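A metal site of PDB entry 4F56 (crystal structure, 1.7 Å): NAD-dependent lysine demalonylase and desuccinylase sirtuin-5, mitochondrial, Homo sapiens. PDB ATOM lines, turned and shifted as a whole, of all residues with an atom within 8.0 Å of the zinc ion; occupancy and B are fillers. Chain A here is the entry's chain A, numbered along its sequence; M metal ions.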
ATOM      1  N   ARG A 136     -16.844  -6.900 -15.379  1.00  0.00           N
ATOM      2  CA  ARG A 136     -16.962  -8.283 -14.903  1.00  0.00           C
ATOM      3  C   ARG A 136     -17.754  -8.255 -13.610  1.00  0.00           C
ATOM      4  O   ARG A 136     -17.544  -7.388 -12.753  1.00  0.00           O
ATOM      5  CB  ARG A 136     -15.576  -8.924 -14.667  1.00  0.00           C
ATOM      6  CG  ARG A 136     -15.666 -10.396 -14.226  1.00  0.00           C
ATOM      7  CD  ARG A 136     -14.327 -11.127 -14.280  1.00  0.00           C
ATOM      8  NE  ARG A 136     -13.421 -10.815 -13.164  1.00  0.00           N
ATOM      9  CZ  ARG A 136     -12.341 -10.030 -13.249  1.00  0.00           C
ATOM     10  NH1 ARG A 136     -12.050  -9.437 -14.400  1.00  0.00           N
ATOM     11  NH2 ARG A 136     -11.564  -9.838 -12.194  1.00  0.00           N
ATOM     12  N   CYS A 137     -18.636  -9.219 -13.449  1.00  0.00           N
ATOM     13  CA  CYS A 137     -19.410  -9.311 -12.219  1.00  0.00           C
ATOM     14  C   CYS A 137     -18.616 -10.018 -11.102  1.00  0.00           C
ATOM     15  O   CYS A 137     -18.095 -11.129 -11.279  1.00  0.00           O
ATOM     16  CB  CYS A 137     -20.720 -10.044 -12.497  1.00  0.00           C
ATOM     17  SG  CYS A 137     -21.785 -10.150 -11.043  1.00  0.00           S
ATOM     18  N   THR A 138     -18.526  -9.351  -9.951  1.00  0.00           N
ATOM     19  CA  THR A 138     -17.810  -9.870  -8.783  1.00  0.00           C
ATOM     20  C   THR A 138     -18.530 -11.067  -8.145  1.00  0.00           C
ATOM     21  O   THR A 138     -17.936 -11.822  -7.386  1.00  0.00           O
ATOM     22  CB  THR A 138     -17.559  -8.778  -7.722  1.00  0.00           C
ATOM     23  OG1 THR A 138     -18.805  -8.200  -7.277  1.00  0.00           O
ATOM     24  CG2 THR A 138     -16.660  -7.691  -8.271  1.00  0.00           C
ATOM     25  N   SER A 139     -19.804 -11.247  -8.487  1.00  0.00           N
ATOM     26  CA  SER A 139     -20.590 -12.350  -7.962  1.00  0.00           C
ATOM     27  C   SER A 139     -20.624 -13.576  -8.910  1.00  0.00           C
ATOM     28  O   SER A 139     -20.236 -14.668  -8.505  1.00  0.00           O
ATOM     29  CB  SER A 139     -21.995 -11.857  -7.585  1.00  0.00           C
ATOM     30  OG  SER A 139     -22.844 -12.944  -7.295  1.00  0.00           O
ATOM     31  N   CYS A 140     -21.068 -13.389 -10.159  1.00  0.00           N
ATOM     32  CA  CYS A 140     -21.209 -14.521 -11.086  1.00  0.00           C
ATOM     33  C   CYS A 140     -20.075 -14.676 -12.118  1.00  0.00           C
ATOM     34  O   CYS A 140     -20.004 -15.680 -12.814  1.00  0.00           O
ATOM     35  CB  CYS A 140     -22.563 -14.455 -11.812  1.00  0.00           C
ATOM     36  SG  CYS A 140     -22.591 -13.261 -13.162  1.00  0.00           S
ATOM     37  N   GLY A 141     -19.202 -13.662 -12.218  1.00  0.00           N
ATOM     38  CA  GLY A 141     -18.034 -13.740 -13.104  1.00  0.00           C
ATOM     39  C   GLY A 141     -18.255 -13.404 -14.576  1.00  0.00           C
ATOM     40  O   GLY A 141     -17.303 -13.409 -15.357  1.00  0.00           O
ATOM     41  N   VAL A 142     -19.492 -13.097 -14.983  1.00  0.00           N
ATOM     42  CA  VAL A 142     -19.755 -12.825 -16.391  1.00  0.00           C
ATOM     43  C   VAL A 142     -18.986 -11.579 -16.850  1.00  0.00           C
ATOM     44  O   VAL A 142     -18.872 -10.607 -16.114  1.00  0.00           O
ATOM     45  CB  VAL A 142     -21.264 -12.688 -16.713  1.00  0.00           C
ATOM     46  CG1 VAL A 142     -21.900 -11.591 -15.892  1.00  0.00           C
ATOM     47  CG2 VAL A 142     -21.494 -12.452 -18.206  1.00  0.00           C
ATOM     48  N   VAL A 143     -18.442 -11.662 -18.054  1.00  0.00           N
ATOM     49  CA  VAL A 143     -17.737 -10.553 -18.661  1.00  0.00           C
ATOM     50  C   VAL A 143     -18.643 -10.025 -19.779  1.00  0.00           C
ATOM     51  O   VAL A 143     -19.155 -10.806 -20.599  1.00  0.00           O
ATOM     52  CB  VAL A 143     -16.355 -10.999 -19.207  1.00  0.00           C
ATOM     53  CG1 VAL A 143     -15.665  -9.847 -19.939  1.00  0.00           C
ATOM     54  CG2 VAL A 143     -15.468 -11.548 -18.078  1.00  0.00           C
ATOM     55  N   ARG A 177     -24.423  -2.577 -11.586  1.00  0.00           N
ATOM     56  CA  ARG A 177     -24.877  -3.886 -11.151  1.00  0.00           C
ATOM     57  C   ARG A 177     -25.120  -4.831 -12.314  1.00  0.00           C
ATOM     58  O   ARG A 177     -25.495  -4.409 -13.409  1.00  0.00           O
ATOM     59  CB  ARG A 177     -26.167  -3.787 -10.307  1.00  0.00           C
ATOM     60  CG  ARG A 177     -26.170  -2.769  -9.190  1.00  0.00           C
ATOM     61  CD  ARG A 177     -25.051  -2.994  -8.166  1.00  0.00           C
ATOM     62  NE  ARG A 177     -25.204  -4.255  -7.434  1.00  0.00           N
ATOM     63  CZ  ARG A 177     -24.703  -4.495  -6.221  1.00  0.00           C
ATOM     64  NH1 ARG A 177     -24.023  -3.553  -5.588  1.00  0.00           N
ATOM     65  NH2 ARG A 177     -24.905  -5.677  -5.643  1.00  0.00           N
ATOM     66  N   CYS A 178     -24.911  -6.112 -12.046  1.00  0.00           N
ATOM     67  CA  CYS A 178     -25.009  -7.165 -13.064  1.00  0.00           C
ATOM     68  C   CYS A 178     -26.458  -7.398 -13.469  1.00  0.00           C
ATOM     69  O   CYS A 178     -27.336  -7.546 -12.617  1.00  0.00           O
ATOM     70  CB  CYS A 178     -24.400  -8.463 -12.517  1.00  0.00           C
ATOM     71  SG  CYS A 178     -24.435  -9.863 -13.661  1.00  0.00           S
ATOM     72  N   GLU A 179     -26.695  -7.405 -14.786  1.00  0.00           N
ATOM     73  CA  GLU A 179     -28.044  -7.557 -15.345  1.00  0.00           C
ATOM     74  C   GLU A 179     -28.241  -8.942 -15.980  1.00  0.00           C
ATOM     75  O   GLU A 179     -29.227  -9.180 -16.664  1.00  0.00           O
ATOM     76  CB  GLU A 179     -28.367  -6.416 -16.334  1.00  0.00           C
ATOM     77  CG  GLU A 179     -28.569  -5.081 -15.639  1.00  0.00           C
ATOM     78  CD  GLU A 179     -28.779  -3.892 -16.582  1.00  0.00           C
ATOM     79  OE1 GLU A 179     -28.956  -4.069 -17.805  1.00  0.00           O
ATOM     80  OE2 GLU A 179     -28.773  -2.751 -16.069  1.00  0.00           O
ATOM     81  N   GLU A 180     -27.299  -9.840 -15.730  1.00  0.00           N
ATOM     82  CA  GLU A 180     -27.381 -11.218 -16.205  1.00  0.00           C
ATOM     83  C   GLU A 180     -28.250 -12.046 -15.253  1.00  0.00           C
ATOM     84  O   GLU A 180     -28.001 -12.060 -14.049  1.00  0.00           O
ATOM     85  CB  GLU A 180     -25.972 -11.825 -16.279  1.00  0.00           C
ATOM     86  CG  GLU A 180     -25.874 -13.213 -16.907  1.00  0.00           C
ATOM     87  CD  GLU A 180     -25.921 -13.188 -18.433  1.00  0.00           C
ATOM     88  OE1 GLU A 180     -25.853 -14.276 -19.049  1.00  0.00           O
ATOM     89  OE2 GLU A 180     -26.020 -12.086 -19.006  1.00  0.00           O
ATOM     90  N   ALA A 181     -29.277 -12.695 -15.797  1.00  0.00           N
ATOM     91  CA  ALA A 181     -30.067 -13.693 -15.045  1.00  0.00           C
ATOM     92  C   ALA A 181     -30.502 -13.219 -13.658  1.00  0.00           C
ATOM     93  O   ALA A 181     -30.437 -13.966 -12.667  1.00  0.00           O
ATOM     94  CB  ALA A 181     -29.293 -15.006 -14.939  1.00  0.00           C
ATOM     95  N   GLY A 182     -30.940 -11.959 -13.599  1.00  0.00           N
ATOM     96  CA  GLY A 182     -31.306 -11.289 -12.352  1.00  0.00           C
ATOM     97  C   GLY A 182     -30.212 -11.211 -11.304  1.00  0.00           C
ATOM     98  O   GLY A 182     -30.495 -10.883 -10.144  1.00  0.00           O
ATOM     99  N   CYS A 183     -28.961 -11.482 -11.696  1.00  0.00           N
ATOM    100  CA  CYS A 183     -27.828 -11.648 -10.742  1.00  0.00           C
ATOM    101  C   CYS A 183     -27.741 -10.534  -9.704  1.00  0.00           C
ATOM    102  O   CYS A 183     -27.722 -10.823  -8.504  1.00  0.00           O
ATOM    103  CB  CYS A 183     -26.482 -11.800 -11.463  1.00  0.00           C
ATOM    104  SG  CYS A 183     -25.023 -11.735 -10.374  1.00  0.00           S
ATOM    105  N   GLY A 184     -27.676  -9.290 -10.155  1.00  0.00           N
ATOM    106  CA  GLY A 184     -27.671  -8.145  -9.264  1.00  0.00           C
ATOM    107  C   GLY A 184     -26.320  -7.814  -8.631  1.00  0.00           C
ATOM    108  O   GLY A 184     -26.200  -6.816  -7.925  1.00  0.00           O
ATOM    109  N   GLY A 185     -25.315  -8.652  -8.890  1.00  0.00           N
ATOM    110  CA  GLY A 185     -23.985  -8.505  -8.301  1.00  0.00           C
ATOM    111  C   GLY A 185     -23.288  -7.213  -8.673  1.00  0.00           C
ATOM    112  O   GLY A 185     -23.611  -6.587  -9.677  1.00  0.00           O
ATOM    113  N   LEU A 186     -22.325  -6.803  -7.852  1.00  0.00           N
ATOM    114  CA  LEU A 186     -21.587  -5.581  -8.123  1.00  0.00           C
ATOM    115  C   LEU A 186     -20.581  -5.842  -9.243  1.00  0.00           C
ATOM    116  O   LEU A 186     -19.786  -6.781  -9.173  1.00  0.00           O
ATOM    117  CB  LEU A 186     -20.863  -5.128  -6.851  1.00  0.00           C
ATOM    118  CG  LEU A 186     -19.848  -3.976  -6.936  1.00  0.00           C
ATOM    119  CD1 LEU A 186     -20.502  -2.661  -7.352  1.00  0.00           C
ATOM    120  CD2 LEU A 186     -19.144  -3.838  -5.597  1.00  0.00           C
ATOM    121  N   LEU A 187     -20.626  -4.995 -10.269  1.00  0.00           N
ATOM    122  CA  LEU A 187     -19.656  -5.063 -11.367  1.00  0.00           C
ATOM    123  C   LEU A 187     -18.384  -4.321 -11.019  1.00  0.00           C
ATOM    124  O   LEU A 187     -18.374  -3.338 -10.260  1.00  0.00           O
ATOM    125  CB  LEU A 187     -20.246  -4.447 -12.657  1.00  0.00           C
ATOM    126  CG  LEU A 187     -21.542  -5.036 -13.221  1.00  0.00           C
ATOM    127  CD1 LEU A 187     -21.988  -4.318 -14.502  1.00  0.00           C
ATOM    128  CD2 LEU A 187     -21.418  -6.549 -13.413  1.00  0.00           C
HETATM  129 ZN    ZN M   1     -23.413 -11.341 -12.091  1.00  0.00          ZN
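N of Cys 137 lies within hydrogen-bond range of O of Val 142.
The side-chain sulfur of Cys 137 lies close to the backbone NH of Ser 139, 3.4 Å away.
The backbone NH (N) of Val 142 sits close to the side-chain sulfur (SG) of Cys 140 (3.6 Å).
The backbone carbonyl oxygen (O) of Gly 185 sits at hydrogen-bond distance from the backbone NH (N) of Cys 178 (2.7 Å).
The side-chain sulfur (SG) of Cys 178 lies close to the backbone NH (N) of Glu 180, at 3.5 Å.
N of Gly 184 sits at hydrogen-bond distance from O of Cys 178, 3.0 Å away.
The side-chain sulfur (SG) of Cys 183 sits close to the backbone NH (N) of Gly 185 (3.4 Å).
Four residues have an atom within 4 Å of the zinc ion: Cys 137, Cys 140, Cys 178 and Cys 183.
Along chain A the residues within 4 Å of the zinc ion span positions 137 to 183.
The nearest printed residue that does not touch the zinc ion is Val 142 (4.1 Å).
The zinc ion is bound by SG of Cys 137 (2.3 Å), SG of Cys 140 (2.3 Å), SG of Cys 178 (2.4 Å) and SG of Cys 183 (2.4 Å).
The zinc ion has four donor atoms within binding distance.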
